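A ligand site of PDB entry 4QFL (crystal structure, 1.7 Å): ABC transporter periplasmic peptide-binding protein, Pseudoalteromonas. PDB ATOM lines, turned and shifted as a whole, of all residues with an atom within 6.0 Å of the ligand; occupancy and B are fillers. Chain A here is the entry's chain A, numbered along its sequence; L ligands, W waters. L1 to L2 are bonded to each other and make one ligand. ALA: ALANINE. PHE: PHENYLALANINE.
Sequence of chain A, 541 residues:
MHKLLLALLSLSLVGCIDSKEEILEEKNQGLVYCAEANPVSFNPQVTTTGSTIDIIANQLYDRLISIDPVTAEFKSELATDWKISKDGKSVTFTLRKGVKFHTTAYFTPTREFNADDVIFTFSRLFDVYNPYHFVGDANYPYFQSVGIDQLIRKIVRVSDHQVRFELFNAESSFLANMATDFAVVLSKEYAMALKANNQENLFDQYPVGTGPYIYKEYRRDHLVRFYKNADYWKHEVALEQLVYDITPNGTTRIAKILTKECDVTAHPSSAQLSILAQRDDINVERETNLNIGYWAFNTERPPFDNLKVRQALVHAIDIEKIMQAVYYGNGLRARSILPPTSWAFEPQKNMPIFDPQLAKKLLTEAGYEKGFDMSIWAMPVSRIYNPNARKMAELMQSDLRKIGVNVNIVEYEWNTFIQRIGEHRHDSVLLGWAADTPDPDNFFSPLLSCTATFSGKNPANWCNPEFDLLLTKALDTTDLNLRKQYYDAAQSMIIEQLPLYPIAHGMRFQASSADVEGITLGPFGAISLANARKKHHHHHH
The side-chain amide nitrogen of Asn 442 lies close to the backbone NH of Asp 436 (2.8 Å). NE1 of Trp 433 lies close to ND2 of Asn 442. The side-chain hydroxyl of Tyr 294 sits close to the backbone NH of Gly 432, at 3.4 Å. The backbone carbonyl oxygen of Leu 431 sits at hydrogen-bond distance from the backbone NH of Tyr 294 (3.0 Å). OG of Ser 51 sits at hydrogen-bond distance from NE1 of Trp 414 (2.7 Å).
An oxygen (O) of PHE L2 lies within hydrogen-bond range of the side-chain hydroxyl of Tyr 385 (2.6 Å). N of Ala 434 is in hydrogen-bond range of O of ALA L1. O of Ala 434 sits at hydrogen-bond distance from N of ALA L1 (2.8 Å). An oxygen (OXT) of PHE L2 lies within hydrogen-bond range of the backbone NH (N) of Gly 50 (2.8 Å). The side-chain carboxylate (OD1) of Asp 436 is in salt-bridge range of a nitrogen (N) of ALA L1 (2.8 Å). N of PHE L2 is in hydrogen-bond range of O of Thr 48 (2.9 Å). An oxygen (O) of PHE L2 is in salt-bridge range of the guanidinium group (NE) of Arg 383 (3.0 Å).
C of Thr 49 touches OXT of PHE L2, at 3.9 Å. CZ2 of Trp 414 touches O of PHE L2, 3.8 Å away. CD1 of Ile 418 touches CD2 of PHE L2 (3.9 Å). CD2 of Leu 431 touches CD1 of PHE L2, 3.6 Å away. Gly 432 touches the ligand. CZ2 of Trp 433 touches N of ALA L1 (3.1 Å). Hydrophobic or aromatic side chains that line the ligand: Tyr 385, Trp 414, Ile 418, Leu 431, Trp 433 and Ala 434. Within 4 Å of the ligand: Thr 48, Thr 49, Gly 50, Arg 383, Tyr 385, Trp 414, Ile 418, Leu 431, Gly 432, Trp 433, Ala 434 and Asp 436.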
ATOM      1  N   THR A  48     -22.379  -8.871  14.713  1.00  0.00           N
ATOM      2  CA  THR A  48     -22.603  -7.744  13.825  1.00  0.00           C
ATOM      3  C   THR A  48     -23.847  -7.972  12.977  1.00  0.00           C
ATOM      4  O   THR A  48     -24.017  -7.347  11.940  1.00  0.00           O
ATOM      5  CB  THR A  48     -21.417  -7.499  12.883  1.00  0.00           C
ATOM      6  OG1 THR A  48     -21.212  -8.648  12.065  1.00  0.00           O
ATOM      7  CG2 THR A  48     -20.170  -7.199  13.677  1.00  0.00           C
ATOM      8  N   THR A  49     -24.730  -8.864  13.422  1.00  0.00           N
ATOM      9  CA  THR A  49     -25.928  -9.119  12.640  1.00  0.00           C
ATOM     10  C   THR A  49     -27.097  -8.248  13.040  1.00  0.00           C
ATOM     11  O   THR A  49     -27.562  -8.283  14.160  1.00  0.00           O
ATOM     12  CB  THR A  49     -26.364 -10.570  12.741  1.00  0.00           C
ATOM     13  OG1 THR A  49     -25.323 -11.391  12.199  1.00  0.00           O
ATOM     14  CG2 THR A  49     -27.656 -10.783  11.968  1.00  0.00           C
ATOM     15  N   GLY A  50     -27.583  -7.452  12.084  1.00  0.00           N
ATOM     16  CA  GLY A  50     -28.612  -6.471  12.372  1.00  0.00           C
ATOM     17  C   GLY A  50     -29.891  -7.044  12.959  1.00  0.00           C
ATOM     18  O   GLY A  50     -30.532  -6.406  13.799  1.00  0.00           O
ATOM     19  N   SER A  51     -30.256  -8.250  12.528  1.00  0.00           N
ATOM     20  CA  SER A  51     -31.450  -8.926  13.012  1.00  0.00           C
ATOM     21  C   SER A  51     -31.417  -9.069  14.518  1.00  0.00           C
ATOM     22  O   SER A  51     -32.422  -8.871  15.182  1.00  0.00           O
ATOM     23  CB  SER A  51     -31.534 -10.306  12.375  1.00  0.00           C
ATOM     24  OG  SER A  51     -31.160 -10.223  11.020  1.00  0.00           O
ATOM     25  N   ILE A  53     -29.305  -7.292  16.656  1.00  0.00           N
ATOM     26  CA  ILE A  53     -29.190  -5.959  17.243  1.00  0.00           C
ATOM     27  C   ILE A  53     -30.515  -5.203  17.246  1.00  0.00           C
ATOM     28  O   ILE A  53     -30.832  -4.455  18.185  1.00  0.00           O
ATOM     29  CB  ILE A  53     -28.104  -5.111  16.523  1.00  0.00           C
ATOM     30  CG1 ILE A  53     -26.742  -5.810  16.606  1.00  0.00           C
ATOM     31  CG2 ILE A  53     -28.027  -3.734  17.128  1.00  0.00           C
ATOM     32  CD1 ILE A  53     -26.311  -6.158  18.018  1.00  0.00           C
ATOM     33  N   PHE A 182     -23.099  -1.761  19.178  1.00  0.00           N
ATOM     34  CA  PHE A 182     -22.300  -2.825  19.788  1.00  0.00           C
ATOM     35  C   PHE A 182     -21.672  -2.357  21.094  1.00  0.00           C
ATOM     36  O   PHE A 182     -21.271  -3.176  21.938  1.00  0.00           O
ATOM     37  CB  PHE A 182     -21.221  -3.303  18.815  1.00  0.00           C
ATOM     38  CG  PHE A 182     -21.716  -3.473  17.400  1.00  0.00           C
ATOM     39  CD1 PHE A 182     -22.603  -4.489  17.085  1.00  0.00           C
ATOM     40  CD2 PHE A 182     -21.323  -2.606  16.398  1.00  0.00           C
ATOM     41  CE1 PHE A 182     -23.072  -4.638  15.801  1.00  0.00           C
ATOM     42  CE2 PHE A 182     -21.781  -2.757  15.106  1.00  0.00           C
ATOM     43  CZ  PHE A 182     -22.660  -3.765  14.811  1.00  0.00           C
ATOM     44  N   TYR A 294     -23.753  -5.657  -2.308  1.00  0.00           N
ATOM     45  CA  TYR A 294     -22.658  -6.043  -3.218  1.00  0.00           C
ATOM     46  C   TYR A 294     -22.635  -7.542  -3.543  1.00  0.00           C
ATOM     47  O   TYR A 294     -23.286  -8.354  -2.899  1.00  0.00           O
ATOM     48  CB  TYR A 294     -21.291  -5.614  -2.637  1.00  0.00           C
ATOM     49  CG  TYR A 294     -21.060  -6.167  -1.254  1.00  0.00           C
ATOM     50  CD1 TYR A 294     -20.912  -7.529  -1.042  1.00  0.00           C
ATOM     51  CD2 TYR A 294     -21.018  -5.327  -0.154  1.00  0.00           C
ATOM     52  CE1 TYR A 294     -20.722  -8.047   0.232  1.00  0.00           C
ATOM     53  CE2 TYR A 294     -20.833  -5.837   1.123  1.00  0.00           C
ATOM     54  CZ  TYR A 294     -20.696  -7.193   1.306  1.00  0.00           C
ATOM     55  OH  TYR A 294     -20.510  -7.692   2.557  1.00  0.00           O
ATOM     56  N   MET A 379     -28.742 -14.538   0.473  1.00  0.00           N
ATOM     57  CA  MET A 379     -29.391 -14.337   1.774  1.00  0.00           C
ATOM     58  C   MET A 379     -30.851 -14.804   1.750  1.00  0.00           C
ATOM     59  O   MET A 379     -31.555 -14.608   0.760  1.00  0.00           O
ATOM     60  CB  MET A 379     -29.314 -12.850   2.172  1.00  0.00           C
ATOM     61  CG  MET A 379     -27.900 -12.328   2.179  1.00  0.00           C
ATOM     62  SD  MET A 379     -27.761 -10.563   2.512  1.00  0.00           S
ATOM     63  CE  MET A 379     -28.270  -9.901   0.939  1.00  0.00           C
ATOM     64  N   ARG A 383     -33.006  -7.532   3.433  1.00  0.00           N
ATOM     65  CA  ARG A 383     -32.184  -6.561   4.156  1.00  0.00           C
ATOM     66  C   ARG A 383     -32.357  -5.222   3.467  1.00  0.00           C
ATOM     67  O   ARG A 383     -32.794  -5.156   2.320  1.00  0.00           O
ATOM     68  CB  ARG A 383     -30.693  -6.935   4.118  1.00  0.00           C
ATOM     69  CG  ARG A 383     -30.367  -8.413   4.230  1.00  0.00           C
ATOM     70  CD  ARG A 383     -30.857  -8.998   5.533  1.00  0.00           C
ATOM     71  NE  ARG A 383     -30.341  -8.294   6.706  1.00  0.00           N
ATOM     72  CZ  ARG A 383     -31.066  -7.981   7.784  1.00  0.00           C
ATOM     73  NH1 ARG A 383     -32.362  -8.267   7.832  1.00  0.00           N
ATOM     74  NH2 ARG A 383     -30.497  -7.349   8.790  1.00  0.00           N
ATOM     75  N   TYR A 385     -30.179  -3.332   2.185  1.00  0.00           N
ATOM     76  CA  TYR A 385     -29.351  -3.227   0.993  1.00  0.00           C
ATOM     77  C   TYR A 385     -29.709  -4.237  -0.083  1.00  0.00           C
ATOM     78  O   TYR A 385     -29.192  -4.164  -1.195  1.00  0.00           O
ATOM     79  CB  TYR A 385     -27.874  -3.344   1.370  1.00  0.00           C
ATOM     80  CG  TYR A 385     -27.565  -4.500   2.293  1.00  0.00           C
ATOM     81  CD1 TYR A 385     -27.317  -5.761   1.774  1.00  0.00           C
ATOM     82  CD2 TYR A 385     -27.527  -4.330   3.662  1.00  0.00           C
ATOM     83  CE1 TYR A 385     -27.022  -6.826   2.604  1.00  0.00           C
ATOM     84  CE2 TYR A 385     -27.243  -5.392   4.501  1.00  0.00           C
ATOM     85  CZ  TYR A 385     -26.993  -6.633   3.967  1.00  0.00           C
ATOM     86  OH  TYR A 385     -26.704  -7.699   4.790  1.00  0.00           O
ATOM     87  N   TRP A 414     -30.593 -17.551   7.941  1.00  0.00           N
ATOM     88  CA  TRP A 414     -29.823 -16.310   8.025  1.00  0.00           C
ATOM     89  C   TRP A 414     -28.582 -16.389   8.882  1.00  0.00           C
ATOM     90  O   TRP A 414     -27.489 -16.122   8.408  1.00  0.00           O
ATOM     91  CB  TRP A 414     -30.723 -15.185   8.514  1.00  0.00           C
ATOM     92  CG  TRP A 414     -30.118 -13.796   8.612  1.00  0.00           C
ATOM     93  CD1 TRP A 414     -30.368 -12.886   9.597  1.00  0.00           C
ATOM     94  CD2 TRP A 414     -29.233 -13.140   7.684  1.00  0.00           C
ATOM     95  NE1 TRP A 414     -29.689 -11.731   9.360  1.00  0.00           N
ATOM     96  CE2 TRP A 414     -28.987 -11.850   8.194  1.00  0.00           C
ATOM     97  CE3 TRP A 414     -28.622 -13.516   6.493  1.00  0.00           C
ATOM     98  CZ2 TRP A 414     -28.155 -10.927   7.547  1.00  0.00           C
ATOM     99  CZ3 TRP A 414     -27.792 -12.607   5.847  1.00  0.00           C
ATOM    100  CH2 TRP A 414     -27.568 -11.317   6.388  1.00  0.00           C
ATOM    101  N   ILE A 418     -24.550 -16.526   7.647  1.00  0.00           N
ATOM    102  CA  ILE A 418     -23.492 -15.606   8.069  1.00  0.00           C
ATOM    103  C   ILE A 418     -22.260 -16.378   8.511  1.00  0.00           C
ATOM    104  O   ILE A 418     -21.127 -16.073   8.145  1.00  0.00           O
ATOM    105  CB  ILE A 418     -23.974 -14.693   9.213  1.00  0.00           C
ATOM    106  CG1 ILE A 418     -25.105 -13.781   8.740  1.00  0.00           C
ATOM    107  CG2 ILE A 418     -22.802 -13.879   9.777  1.00  0.00           C
ATOM    108  CD1 ILE A 418     -24.743 -12.959   7.573  1.00  0.00           C
ATOM    109  N   LEU A 431     -24.273 -10.075  -0.458  1.00  0.00           N
ATOM    110  CA  LEU A 431     -24.362  -9.571   0.904  1.00  0.00           C
ATOM    111  C   LEU A 431     -24.321  -8.048   0.872  1.00  0.00           C
ATOM    112  O   LEU A 431     -24.667  -7.436  -0.128  1.00  0.00           O
ATOM    113  CB  LEU A 431     -23.214 -10.121   1.752  1.00  0.00           C
ATOM    114  CG  LEU A 431     -23.633 -10.982   2.940  1.00  0.00           C
ATOM    115  CD1 LEU A 431     -22.491 -11.805   3.504  1.00  0.00           C
ATOM    116  CD2 LEU A 431     -24.292 -10.139   4.020  1.00  0.00           C
ATOM    117  N   GLY A 432     -23.882  -7.445   1.955  1.00  0.00           N
ATOM    118  CA  GLY A 432     -23.767  -5.995   1.993  1.00  0.00           C
ATOM    119  C   GLY A 432     -23.552  -5.506   3.408  1.00  0.00           C
ATOM    120  O   GLY A 432     -23.140  -6.258   4.280  1.00  0.00           O
ATOM    121  N   TRP A 433     -23.823  -4.230   3.626  1.00  0.00           N
ATOM    122  CA  TRP A 433     -23.611  -3.647   4.927  1.00  0.00           C
ATOM    123  C   TRP A 433     -24.606  -2.530   5.135  1.00  0.00           C
ATOM    124  O   TRP A 433     -24.786  -1.666   4.268  1.00  0.00           O
ATOM    125  CB  TRP A 433     -22.201  -3.095   5.002  1.00  0.00           C
ATOM    126  CG  TRP A 433     -21.743  -2.640   6.353  1.00  0.00           C
ATOM    127  CD1 TRP A 433     -21.450  -1.353   6.724  1.00  0.00           C
ATOM    128  CD2 TRP A 433     -21.485  -3.458   7.502  1.00  0.00           C
ATOM    129  NE1 TRP A 433     -21.039  -1.329   8.031  1.00  0.00           N
ATOM    130  CE2 TRP A 433     -21.046  -2.603   8.530  1.00  0.00           C
ATOM    131  CE3 TRP A 433     -21.575  -4.823   7.761  1.00  0.00           C
ATOM    132  CZ2 TRP A 433     -20.710  -3.078   9.802  1.00  0.00           C
ATOM    133  CZ3 TRP A 433     -21.238  -5.297   9.033  1.00  0.00           C
ATOM    134  CH2 TRP A 433     -20.816  -4.424  10.023  1.00  0.00           C
ATOM    135  N   ALA A 434     -25.278  -2.555   6.278  1.00  0.00           N
ATOM    136  CA  ALA A 434     -26.056  -1.417   6.721  1.00  0.00           C
ATOM    137  C   ALA A 434     -25.233  -0.608   7.752  1.00  0.00           C
ATOM    138  O   ALA A 434     -24.939  -1.079   8.841  1.00  0.00           O
ATOM    139  CB  ALA A 434     -27.377  -1.881   7.315  1.00  0.00           C
ATOM    140  N   ALA A 435     -24.846   0.591   7.375  1.00  0.00           N
ATOM    141  CA  ALA A 435     -23.924   1.378   8.176  1.00  0.00           C
ATOM    142  C   ALA A 435     -24.375   1.577   9.625  1.00  0.00           C
ATOM    143  O   ALA A 435     -25.563   1.801   9.898  1.00  0.00           O
ATOM    144  CB  ALA A 435     -23.645   2.722   7.512  1.00  0.00           C
ATOM    145  N   ASP A 436     -23.418   1.496  10.553  1.00  0.00           N
ATOM    146  CA  ASP A 436     -23.697   1.681  11.969  1.00  0.00           C
ATOM    147  C   ASP A 436     -23.541   3.150  12.368  1.00  0.00           C
ATOM    148  O   ASP A 436     -24.125   3.611  13.358  1.00  0.00           O
ATOM    149  CB  ASP A 436     -22.764   0.818  12.827  1.00  0.00           C
ATOM    150  CG  ASP A 436     -22.622  -0.608  12.305  1.00  0.00           C
ATOM    151  OD1 ASP A 436     -23.603  -1.383  12.367  1.00  0.00           O
ATOM    152  OD2 ASP A 436     -21.509  -0.967  11.851  1.00  0.00           O
ATOM    153  N   ASN A 442     -16.681   3.227   8.550  1.00  0.00           N
ATOM    154  CA  ASN A 442     -17.606   2.129   8.853  1.00  0.00           C
ATOM    155  C   ASN A 442     -17.939   1.250   7.640  1.00  0.00           C
ATOM    156  O   ASN A 442     -18.381   0.106   7.779  1.00  0.00           O
ATOM    157  CB  ASN A 442     -18.870   2.661   9.538  1.00  0.00           C
ATOM    158  CG  ASN A 442     -19.769   1.549  10.089  1.00  0.00           C
ATOM    159  OD1 ASN A 442     -19.440   0.904  11.089  1.00  0.00           O
ATOM    160  ND2 ASN A 442     -20.897   1.331   9.455  1.00  0.00           N
ATOM    161  N   LEU A 447     -15.299  -4.273   7.048  1.00  0.00           N
ATOM    162  CA  LEU A 447     -15.714  -5.047   5.885  1.00  0.00           C
ATOM    163  C   LEU A 447     -14.556  -5.651   5.145  1.00  0.00           C
ATOM    164  O   LEU A 447     -14.490  -6.858   4.960  1.00  0.00           O
ATOM    165  CB  LEU A 447     -16.442  -4.142   4.903  1.00  0.00           C
ATOM    166  CG  LEU A 447     -17.930  -4.391   4.694  1.00  0.00           C
ATOM    167  CD1 LEU A 447     -18.643  -4.349   6.034  1.00  0.00           C
ATOM    168  CD2 LEU A 447     -18.482  -3.364   3.736  1.00  0.00           C
ATOM    169  N   LYS A 457     -15.239 -11.756   8.937  1.00  0.00           N
ATOM    170  CA  LYS A 457     -16.299 -10.806   8.612  1.00  0.00           C
ATOM    171  C   LYS A 457     -16.145 -10.146   7.243  1.00  0.00           C
ATOM    172  O   LYS A 457     -16.920  -9.264   6.872  1.00  0.00           O
ATOM    173  CB  LYS A 457     -16.422  -9.740   9.712  1.00  0.00           C
ATOM    174  CG  LYS A 457     -16.979 -10.306  11.028  1.00  0.00           C
ATOM    175  CD  LYS A 457     -18.202 -11.203  10.774  1.00  0.00           C
ATOM    176  CE  LYS A 457     -19.024 -11.402  12.026  1.00  0.00           C
ATOM    177  NZ  LYS A 457     -20.071 -12.420  11.800  1.00  0.00           N
ATOM    178  N   ASN A 458     -15.138 -10.581   6.480  1.00  0.00           N
ATOM    179  CA  ASN A 458     -14.877 -10.039   5.155  1.00  0.00           C
ATOM    180  C   ASN A 458     -15.349 -11.030   4.091  1.00  0.00           C
ATOM    181  O   ASN A 458     -14.688 -12.025   3.853  1.00  0.00           O
ATOM    182  CB  ASN A 458     -13.380  -9.786   5.012  1.00  0.00           C
ATOM    183  CG  ASN A 458     -13.004  -9.212   3.673  1.00  0.00           C
ATOM    184  OD1 ASN A 458     -13.789  -9.223   2.725  1.00  0.00           O
ATOM    185  ND2 ASN A 458     -11.794  -8.697   3.574  1.00  0.00           N
ATOM    186  N   PRO A 459     -16.500 -10.763   3.454  1.00  0.00           N
ATOM    187  CA  PRO A 459     -17.069 -11.738   2.518  1.00  0.00           C
ATOM    188  C   PRO A 459     -16.218 -11.933   1.262  1.00  0.00           C
ATOM    189  O   PRO A 459     -16.426 -12.896   0.537  1.00  0.00           O
ATOM    190  CB  PRO A 459     -18.444 -11.129   2.167  1.00  0.00           C
ATOM    191  CG  PRO A 459     -18.721 -10.152   3.249  1.00  0.00           C
ATOM    192  CD  PRO A 459     -17.390  -9.602   3.666  1.00  0.00           C
HETATM  193  N   ALA L   1     -23.754  -3.201  10.209  1.00  0.00           N
HETATM  194  CA  ALA L   1     -24.354  -4.485  10.539  1.00  0.00           C
HETATM  195  C   ALA L   1     -24.868  -5.192   9.288  1.00  0.00           C
HETATM  196  O   ALA L   1     -25.258  -4.534   8.322  1.00  0.00           O
HETATM  197  CB  ALA L   1     -25.487  -4.310  11.560  1.00  0.00           C
HETATM  198  N   PHE L   2     -24.864  -6.524   9.294  1.00  0.00           N
HETATM  199  CA  PHE L   2     -25.424  -7.311   8.208  1.00  0.00           C
HETATM  200  C   PHE L   2     -26.934  -7.218   8.227  1.00  0.00           C
HETATM  201  O   PHE L   2     -27.582  -7.225   7.184  1.00  0.00           O
HETATM  202  CB  PHE L   2     -25.025  -8.774   8.350  1.00  0.00           C
HETATM  203  CG  PHE L   2     -23.593  -9.042   8.064  1.00  0.00           C
HETATM  204  CD1 PHE L   2     -22.997  -8.538   6.921  1.00  0.00           C
HETATM  205  CD2 PHE L   2     -22.837  -9.800   8.932  1.00  0.00           C
HETATM  206  CE1 PHE L   2     -21.674  -8.796   6.645  1.00  0.00           C
HETATM  207  CE2 PHE L   2     -21.521 -10.063   8.661  1.00  0.00           C
HETATM  208  CZ  PHE L   2     -20.935  -9.557   7.527  1.00  0.00           C
HETATM  209  OXT PHE L   2     -27.544  -7.154   9.295  1.00  0.00           O
HETATM  210  O   HOH W   1     -18.713  -7.249   7.197  1.00  0.00           O
